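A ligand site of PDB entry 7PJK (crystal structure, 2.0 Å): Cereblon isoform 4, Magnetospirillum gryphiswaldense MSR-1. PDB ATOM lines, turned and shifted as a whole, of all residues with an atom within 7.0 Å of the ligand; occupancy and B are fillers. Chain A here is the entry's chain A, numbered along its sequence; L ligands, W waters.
O of Phe 78 lies within hydrogen-bond range of N1 of the ligand, at 3.0 Å.
OH of Tyr 102 lies within hydrogen-bond range of O1 of the ligand, at 2.8 Å.
The backbone NH (N) of Trp 80 sits close to an oxygen (O1) of the ligand.
The side-chain amide oxygen (OD1) of Asn 51 is in hydrogen-bond range of the backbone NH (N) of Ala 53, at 3.0 Å.
The side-chain hydroxyl (OG) of Ser 79 sits at hydrogen-bond distance from the backbone carbonyl oxygen (O) of Phe 81 (2.9 Å).
The indole nitrogen of Trp 80 is in hydrogen-bond range of the backbone carbonyl oxygen of Phe 50 (2.9 Å).
The side-chain hydroxyl (OG) of Ser 79 lies within hydrogen-bond range of the backbone carbonyl oxygen (O) of Tyr 84, 2.9 Å away.
NE1 of Trp 86 lies within hydrogen-bond range of O of Glu 77, at 2.8 Å.
The backbone NH (N) of Trp 86 lies within hydrogen-bond range of the backbone carbonyl oxygen (O) of Ser 75, at 2.7 Å.
The side-chain amide oxygen of Asn 51 is in hydrogen-bond range of the backbone NH of Met 55, 3.0 Å away.
CB of Asn 51 touches N4 of the ligand, at 3.4 Å.
Pro 52 touches the ligand (CD to O2, 3.5 Å).
CA of Ser 79 touches O1 of the ligand, 3.5 Å away.
Trp 86 touches the ligand.
NE1 of Trp 100 touches C7 of the ligand (3.4 Å).
Of the 22 residues printed, 8 come within 4 Å of the ligand.
Water W1 lies within hydrogen-bond range of NE1 of Trp 100 and N4 of the ligand.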
ATOM      1  N   VAL A  49     -20.598  29.590  26.155  1.00  0.00           N
ATOM      2  CA  VAL A  49     -20.322  28.691  25.004  1.00  0.00           C
ATOM      3  C   VAL A  49     -20.399  29.500  23.711  1.00  0.00           C
ATOM      4  O   VAL A  49     -21.045  30.567  23.723  1.00  0.00           O
ATOM      5  CB  VAL A  49     -21.311  27.500  24.991  1.00  0.00           C
ATOM      6  CG1 VAL A  49     -21.132  26.624  26.220  1.00  0.00           C
ATOM      7  CG2 VAL A  49     -22.755  27.955  24.874  1.00  0.00           C
ATOM      8  N   PHE A  50     -19.766  29.009  22.638  1.00  0.00           N
ATOM      9  CA  PHE A  50     -19.881  29.549  21.255  1.00  0.00           C
ATOM     10  C   PHE A  50     -20.361  28.437  20.317  1.00  0.00           C
ATOM     11  O   PHE A  50     -19.890  27.299  20.447  1.00  0.00           O
ATOM     12  CB  PHE A  50     -18.535  30.054  20.737  1.00  0.00           C
ATOM     13  CG  PHE A  50     -18.018  31.333  21.344  1.00  0.00           C
ATOM     14  CD1 PHE A  50     -17.136  31.306  22.407  1.00  0.00           C
ATOM     15  CD2 PHE A  50     -18.374  32.554  20.802  1.00  0.00           C
ATOM     16  CE1 PHE A  50     -16.645  32.489  22.946  1.00  0.00           C
ATOM     17  CE2 PHE A  50     -17.875  33.738  21.347  1.00  0.00           C
ATOM     18  CZ  PHE A  50     -17.020  33.700  22.416  1.00  0.00           C
ATOM     19  N   ASN A  51     -21.244  28.785  19.374  1.00  0.00           N
ATOM     20  CA  ASN A  51     -21.749  27.854  18.331  1.00  0.00           C
ATOM     21  C   ASN A  51     -20.840  27.980  17.099  1.00  0.00           C
ATOM     22  O   ASN A  51     -19.949  28.831  17.070  1.00  0.00           O
ATOM     23  CB  ASN A  51     -23.242  28.088  18.077  1.00  0.00           C
ATOM     24  CG  ASN A  51     -23.559  29.334  17.281  1.00  0.00           C
ATOM     25  OD1 ASN A  51     -22.669  30.032  16.802  1.00  0.00           O
ATOM     26  ND2 ASN A  51     -24.842  29.609  17.105  1.00  0.00           N
ATOM     27  N   PRO A  52     -20.997  27.107  16.075  1.00  0.00           N
ATOM     28  CA  PRO A  52     -20.147  27.148  14.891  1.00  0.00           C
ATOM     29  C   PRO A  52     -20.273  28.445  14.074  1.00  0.00           C
ATOM     30  O   PRO A  52     -19.387  28.707  13.275  1.00  0.00           O
ATOM     31  CB  PRO A  52     -20.599  25.954  14.052  1.00  0.00           C
ATOM     32  CG  PRO A  52     -21.350  25.048  15.021  1.00  0.00           C
ATOM     33  CD  PRO A  52     -21.964  26.004  16.032  1.00  0.00           C
ATOM     34  N   ALA A  53     -21.344  29.212  14.261  1.00  0.00           N
ATOM     35  CA  ALA A  53     -21.569  30.527  13.619  1.00  0.00           C
ATOM     36  C   ALA A  53     -20.889  31.642  14.427  1.00  0.00           C
ATOM     37  O   ALA A  53     -21.032  32.819  14.045  1.00  0.00           O
ATOM     38  CB  ALA A  53     -23.048  30.792  13.463  1.00  0.00           C
ATOM     39  N   MET A  55     -21.500  32.703  17.464  1.00  0.00           N
ATOM     40  CA  MET A  55     -22.393  33.347  18.459  1.00  0.00           C
ATOM     41  C   MET A  55     -22.023  32.845  19.855  1.00  0.00           C
ATOM     42  O   MET A  55     -21.922  31.612  20.025  1.00  0.00           O
ATOM     43  CB  MET A  55     -23.867  33.028  18.192  1.00  0.00           C
ATOM     44  CG  MET A  55     -24.351  33.494  16.843  1.00  0.00           C
ATOM     45  SD  MET A  55     -26.142  33.293  16.695  1.00  0.00           S
ATOM     46  CE  MET A  55     -26.696  34.514  17.888  1.00  0.00           C
ATOM     47  N   PHE A  57     -23.216  32.422  23.760  1.00  0.00           N
ATOM     48  CA  PHE A  57     -24.392  32.289  24.637  1.00  0.00           C
ATOM     49  C   PHE A  57     -23.900  32.095  26.064  1.00  0.00           C
ATOM     50  O   PHE A  57     -22.967  31.300  26.294  1.00  0.00           O
ATOM     51  CB  PHE A  57     -25.288  31.129  24.201  1.00  0.00           C
ATOM     52  CG  PHE A  57     -25.800  31.221  22.787  1.00  0.00           C
ATOM     53  CD1 PHE A  57     -26.949  31.925  22.496  1.00  0.00           C
ATOM     54  CD2 PHE A  57     -25.121  30.600  21.743  1.00  0.00           C
ATOM     55  CE1 PHE A  57     -27.416  32.030  21.191  1.00  0.00           C
ATOM     56  CE2 PHE A  57     -25.589  30.705  20.438  1.00  0.00           C
ATOM     57  CZ  PHE A  57     -26.732  31.403  20.176  1.00  0.00           C
ATOM     58  N   SER A  75     -29.826  15.810  18.004  1.00  0.00           N
ATOM     59  CA  SER A  75     -28.528  15.774  17.283  1.00  0.00           C
ATOM     60  C   SER A  75     -27.368  15.859  18.277  1.00  0.00           C
ATOM     61  O   SER A  75     -27.475  16.635  19.243  1.00  0.00           O
ATOM     62  CB  SER A  75     -28.467  16.901  16.280  1.00  0.00           C
ATOM     63  OG  SER A  75     -27.186  16.948  15.657  1.00  0.00           O
ATOM     64  N   GLY A  76     -26.306  15.091  18.050  1.00  0.00           N
ATOM     65  CA  GLY A  76     -25.072  15.085  18.865  1.00  0.00           C
ATOM     66  C   GLY A  76     -24.033  16.079  18.347  1.00  0.00           C
ATOM     67  O   GLY A  76     -23.116  16.397  19.118  1.00  0.00           O
ATOM     68  N   GLU A  77     -24.175  16.553  17.104  1.00  0.00           N
ATOM     69  CA  GLU A  77     -23.197  17.446  16.409  1.00  0.00           C
ATOM     70  C   GLU A  77     -23.013  18.749  17.211  1.00  0.00           C
ATOM     71  O   GLU A  77     -24.023  19.424  17.467  1.00  0.00           O
ATOM     72  CB  GLU A  77     -23.664  17.772  14.992  1.00  0.00           C
ATOM     73  CG  GLU A  77     -23.577  16.587  14.041  1.00  0.00           C
ATOM     74  CD  GLU A  77     -24.163  16.812  12.656  1.00  0.00           C
ATOM     75  OE1 GLU A  77     -25.147  17.573  12.542  1.00  0.00           O
ATOM     76  OE2 GLU A  77     -23.629  16.210  11.695  1.00  0.00           O
ATOM     77  N   PHE A  78     -21.779  19.061  17.596  1.00  0.00           N
ATOM     78  CA  PHE A  78     -21.348  20.336  18.222  1.00  0.00           C
ATOM     79  C   PHE A  78     -21.862  20.467  19.665  1.00  0.00           C
ATOM     80  O   PHE A  78     -21.778  21.578  20.204  1.00  0.00           O
ATOM     81  CB  PHE A  78     -21.813  21.542  17.398  1.00  0.00           C
ATOM     82  CG  PHE A  78     -21.384  21.536  15.949  1.00  0.00           C
ATOM     83  CD1 PHE A  78     -20.047  21.564  15.620  1.00  0.00           C
ATOM     84  CD2 PHE A  78     -22.313  21.508  14.928  1.00  0.00           C
ATOM     85  CE1 PHE A  78     -19.636  21.550  14.286  1.00  0.00           C
ATOM     86  CE2 PHE A  78     -21.918  21.492  13.601  1.00  0.00           C
ATOM     87  CZ  PHE A  78     -20.580  21.520  13.289  1.00  0.00           C
ATOM     88  N   SER A  79     -22.379  19.395  20.275  1.00  0.00           N
ATOM     89  CA  SER A  79     -22.941  19.433  21.662  1.00  0.00           C
ATOM     90  C   SER A  79     -21.892  19.982  22.626  1.00  0.00           C
ATOM     91  O   SER A  79     -20.769  19.480  22.632  1.00  0.00           O
ATOM     92  CB  SER A  79     -23.448  18.098  22.112  1.00  0.00           C
ATOM     93  OG  SER A  79     -24.027  18.205  23.406  1.00  0.00           O
ATOM     94  N   TRP A  80     -22.253  20.997  23.419  1.00  0.00           N
ATOM     95  CA  TRP A  80     -21.401  21.607  24.460  1.00  0.00           C
ATOM     96  C   TRP A  80     -21.277  20.675  25.672  1.00  0.00           C
ATOM     97  O   TRP A  80     -20.380  20.905  26.490  1.00  0.00           O
ATOM     98  CB  TRP A  80     -21.966  22.965  24.884  1.00  0.00           C
ATOM     99  CG  TRP A  80     -21.938  23.981  23.791  1.00  0.00           C
ATOM    100  CD1 TRP A  80     -20.874  24.336  23.018  1.00  0.00           C
ATOM    101  CD2 TRP A  80     -23.036  24.790  23.354  1.00  0.00           C
ATOM    102  NE1 TRP A  80     -21.237  25.311  22.126  1.00  0.00           N
ATOM    103  CE2 TRP A  80     -22.556  25.620  22.314  1.00  0.00           C
ATOM    104  CE3 TRP A  80     -24.383  24.918  23.741  1.00  0.00           C
ATOM    105  CZ2 TRP A  80     -23.362  26.542  21.665  1.00  0.00           C
ATOM    106  CZ3 TRP A  80     -25.179  25.827  23.097  1.00  0.00           C
ATOM    107  CH2 TRP A  80     -24.680  26.631  22.068  1.00  0.00           C
ATOM    108  N   PHE A  81     -22.157  19.684  25.784  1.00  0.00           N
ATOM    109  CA  PHE A  81     -22.223  18.756  26.935  1.00  0.00           C
ATOM    110  C   PHE A  81     -22.018  17.332  26.424  1.00  0.00           C
ATOM    111  O   PHE A  81     -22.907  16.790  25.724  1.00  0.00           O
ATOM    112  CB  PHE A  81     -23.536  18.976  27.696  1.00  0.00           C
ATOM    113  CG  PHE A  81     -23.742  20.400  28.138  1.00  0.00           C
ATOM    114  CD1 PHE A  81     -23.132  20.888  29.287  1.00  0.00           C
ATOM    115  CD2 PHE A  81     -24.562  21.256  27.415  1.00  0.00           C
ATOM    116  CE1 PHE A  81     -23.337  22.191  29.712  1.00  0.00           C
ATOM    117  CE2 PHE A  81     -24.763  22.566  27.834  1.00  0.00           C
ATOM    118  CZ  PHE A  81     -24.149  23.026  28.983  1.00  0.00           C
ATOM    119  N   TYR A  84     -24.479  14.101  25.471  1.00  0.00           N
ATOM    120  CA  TYR A  84     -25.854  14.628  25.311  1.00  0.00           C
ATOM    121  C   TYR A  84     -26.113  15.029  23.862  1.00  0.00           C
ATOM    122  O   TYR A  84     -25.231  15.604  23.223  1.00  0.00           O
ATOM    123  CB  TYR A  84     -26.101  15.800  26.264  1.00  0.00           C
ATOM    124  CG  TYR A  84     -26.093  15.440  27.716  1.00  0.00           C
ATOM    125  CD1 TYR A  84     -24.939  15.573  28.479  1.00  0.00           C
ATOM    126  CD2 TYR A  84     -27.230  14.954  28.335  1.00  0.00           C
ATOM    127  CE1 TYR A  84     -24.925  15.248  29.827  1.00  0.00           C
ATOM    128  CE2 TYR A  84     -27.226  14.606  29.683  1.00  0.00           C
ATOM    129  CZ  TYR A  84     -26.075  14.767  30.429  1.00  0.00           C
ATOM    130  OH  TYR A  84     -26.058  14.449  31.754  1.00  0.00           O
ATOM    131  N   TRP A  86     -28.963  17.241  21.458  1.00  0.00           N
ATOM    132  CA  TRP A  86     -29.747  18.485  21.707  1.00  0.00           C
ATOM    133  C   TRP A  86     -30.892  18.616  20.704  1.00  0.00           C
ATOM    134  O   TRP A  86     -30.772  18.146  19.557  1.00  0.00           O
ATOM    135  CB  TRP A  86     -28.838  19.723  21.685  1.00  0.00           C
ATOM    136  CG  TRP A  86     -28.020  19.853  20.444  1.00  0.00           C
ATOM    137  CD1 TRP A  86     -26.729  19.441  20.280  1.00  0.00           C
ATOM    138  CD2 TRP A  86     -28.429  20.421  19.180  1.00  0.00           C
ATOM    139  NE1 TRP A  86     -26.312  19.713  19.008  1.00  0.00           N
ATOM    140  CE2 TRP A  86     -27.329  20.303  18.300  1.00  0.00           C
ATOM    141  CE3 TRP A  86     -29.608  20.985  18.695  1.00  0.00           C
ATOM    142  CZ2 TRP A  86     -27.369  20.746  16.987  1.00  0.00           C
ATOM    143  CZ3 TRP A  86     -29.645  21.436  17.392  1.00  0.00           C
ATOM    144  CH2 TRP A  86     -28.544  21.317  16.547  1.00  0.00           C
ATOM    145  N   THR A  87     -31.966  19.241  21.170  1.00  0.00           N
ATOM    146  CA  THR A  87     -33.105  19.708  20.344  1.00  0.00           C
ATOM    147  C   THR A  87     -33.301  21.196  20.653  1.00  0.00           C
ATOM    148  O   THR A  87     -33.149  21.564  21.832  1.00  0.00           O
ATOM    149  CB  THR A  87     -34.354  18.857  20.627  1.00  0.00           C
ATOM    150  OG1 THR A  87     -33.999  17.489  20.384  1.00  0.00           O
ATOM    151  CG2 THR A  87     -35.544  19.203  19.774  1.00  0.00           C
ATOM    152  N   ILE A  88     -33.571  21.997  19.622  1.00  0.00           N
ATOM    153  CA  ILE A  88     -33.822  23.449  19.753  1.00  0.00           C
ATOM    154  C   ILE A  88     -35.099  23.624  20.594  1.00  0.00           C
ATOM    155  O   ILE A  88     -36.100  22.935  20.295  1.00  0.00           O
ATOM    156  CB  ILE A  88     -33.930  24.133  18.369  1.00  0.00           C
ATOM    157  CG1 ILE A  88     -32.579  24.131  17.653  1.00  0.00           C
ATOM    158  CG2 ILE A  88     -34.510  25.537  18.487  1.00  0.00           C
ATOM    159  CD1 ILE A  88     -32.671  24.310  16.145  1.00  0.00           C
ATOM    160  N   HIS A  97     -36.291  31.804  20.275  1.00  0.00           N
ATOM    161  CA  HIS A  97     -35.300  30.745  20.594  1.00  0.00           C
ATOM    162  C   HIS A  97     -34.764  30.963  22.006  1.00  0.00           C
ATOM    163  O   HIS A  97     -34.026  31.939  22.208  1.00  0.00           O
ATOM    164  CB  HIS A  97     -34.181  30.728  19.546  1.00  0.00           C
ATOM    165  CG  HIS A  97     -33.151  29.674  19.823  1.00  0.00           C
ATOM    166  ND1 HIS A  97     -31.837  29.827  19.470  1.00  0.00           N
ATOM    167  CD2 HIS A  97     -33.253  28.475  20.440  1.00  0.00           C
ATOM    168  CE1 HIS A  97     -31.162  28.766  19.839  1.00  0.00           C
ATOM    169  NE2 HIS A  97     -32.007  27.917  20.440  1.00  0.00           N
ATOM    170  N   GLY A  99     -33.304  28.327  23.970  1.00  0.00           N
ATOM    171  CA  GLY A  99     -32.130  27.468  24.181  1.00  0.00           C
ATOM    172  C   GLY A  99     -32.300  26.083  23.587  1.00  0.00           C
ATOM    173  O   GLY A  99     -32.723  25.981  22.433  1.00  0.00           O
ATOM    174  N   TRP A 100     -31.956  25.047  24.359  1.00  0.00           N
ATOM    175  CA  TRP A 100     -31.892  23.648  23.889  1.00  0.00           C
ATOM    176  C   TRP A 100     -32.331  22.696  25.017  1.00  0.00           C
ATOM    177  O   TRP A 100     -32.063  22.993  26.200  1.00  0.00           O
ATOM    178  CB  TRP A 100     -30.472  23.315  23.382  1.00  0.00           C
ATOM    179  CG  TRP A 100     -29.969  24.254  22.341  1.00  0.00           C
ATOM    180  CD1 TRP A 100     -30.056  24.100  20.975  1.00  0.00           C
ATOM    181  CD2 TRP A 100     -29.311  25.513  22.553  1.00  0.00           C
ATOM    182  NE1 TRP A 100     -29.485  25.171  20.341  1.00  0.00           N
ATOM    183  CE2 TRP A 100     -29.026  26.053  21.281  1.00  0.00           C
ATOM    184  CE3 TRP A 100     -28.937  26.243  23.680  1.00  0.00           C
ATOM    185  CZ2 TRP A 100     -28.395  27.292  21.113  1.00  0.00           C
ATOM    186  CZ3 TRP A 100     -28.316  27.459  23.530  1.00  0.00           C
ATOM    187  CH2 TRP A 100     -28.053  27.982  22.258  1.00  0.00           C
ATOM    188  N   TYR A 102     -31.492  18.846  26.248  1.00  0.00           N
ATOM    189  CA  TYR A 102     -30.413  17.824  26.149  1.00  0.00           C
ATOM    190  C   TYR A 102     -30.957  16.492  26.634  1.00  0.00           C
ATOM    191  O   TYR A 102     -31.702  16.470  27.626  1.00  0.00           O
ATOM    192  CB  TYR A 102     -29.180  18.288  26.915  1.00  0.00           C
ATOM    193  CG  TYR A 102     -28.495  19.466  26.273  1.00  0.00           C
ATOM    194  CD1 TYR A 102     -27.528  19.287  25.298  1.00  0.00           C
ATOM    195  CD2 TYR A 102     -28.832  20.766  26.626  1.00  0.00           C
ATOM    196  CE1 TYR A 102     -26.901  20.366  24.704  1.00  0.00           C
ATOM    197  CE2 TYR A 102     -28.209  21.851  26.037  1.00  0.00           C
ATOM    198  CZ  TYR A 102     -27.244  21.651  25.068  1.00  0.00           C
ATOM    199  OH  TYR A 102     -26.635  22.720  24.468  1.00  0.00           O
HETATM  200  N1  LIG L   1     -24.118  23.350  20.608  1.00  0.00           N
HETATM  201  N2  LIG L   1     -25.209  24.075  16.696  1.00  0.00           N
HETATM  202  C1  LIG L   1     -24.196  24.189  19.505  1.00  0.00           C
HETATM  203  C2  LIG L   1     -25.571  24.614  19.064  1.00  0.00           C
HETATM  204  C3  LIG L   1     -25.322  24.759  15.532  1.00  0.00           C
HETATM  205  C4  LIG L   1     -25.750  26.062  15.839  1.00  0.00           C
HETATM  206  C5  LIG L   1     -25.961  27.020  14.818  1.00  0.00           C
HETATM  207  C6  LIG L   1     -25.287  25.312  13.223  1.00  0.00           C
HETATM  208  C7  LIG L   1     -26.608  23.555  19.398  1.00  0.00           C
HETATM  209  C8  LIG L   1     -26.547  23.194  20.878  1.00  0.00           C
HETATM  210  C9  LIG L   1     -25.165  22.854  21.347  1.00  0.00           C
HETATM  211  N3  LIG L   1     -25.570  24.941  17.641  1.00  0.00           N
HETATM  212  O1  LIG L   1     -24.951  22.196  22.343  1.00  0.00           O
HETATM  213  O2  LIG L   1     -23.194  24.573  18.941  1.00  0.00           O
HETATM  214  N4  LIG L   1     -25.902  26.144  17.174  1.00  0.00           N
HETATM  215  C10 LIG L   1     -25.728  26.620  13.531  1.00  0.00           C
HETATM  216  C11 LIG L   1     -25.092  24.373  14.192  1.00  0.00           C
HETATM  217  O   HOH W   1     -29.341  25.855  17.302  1.00  0.00           O
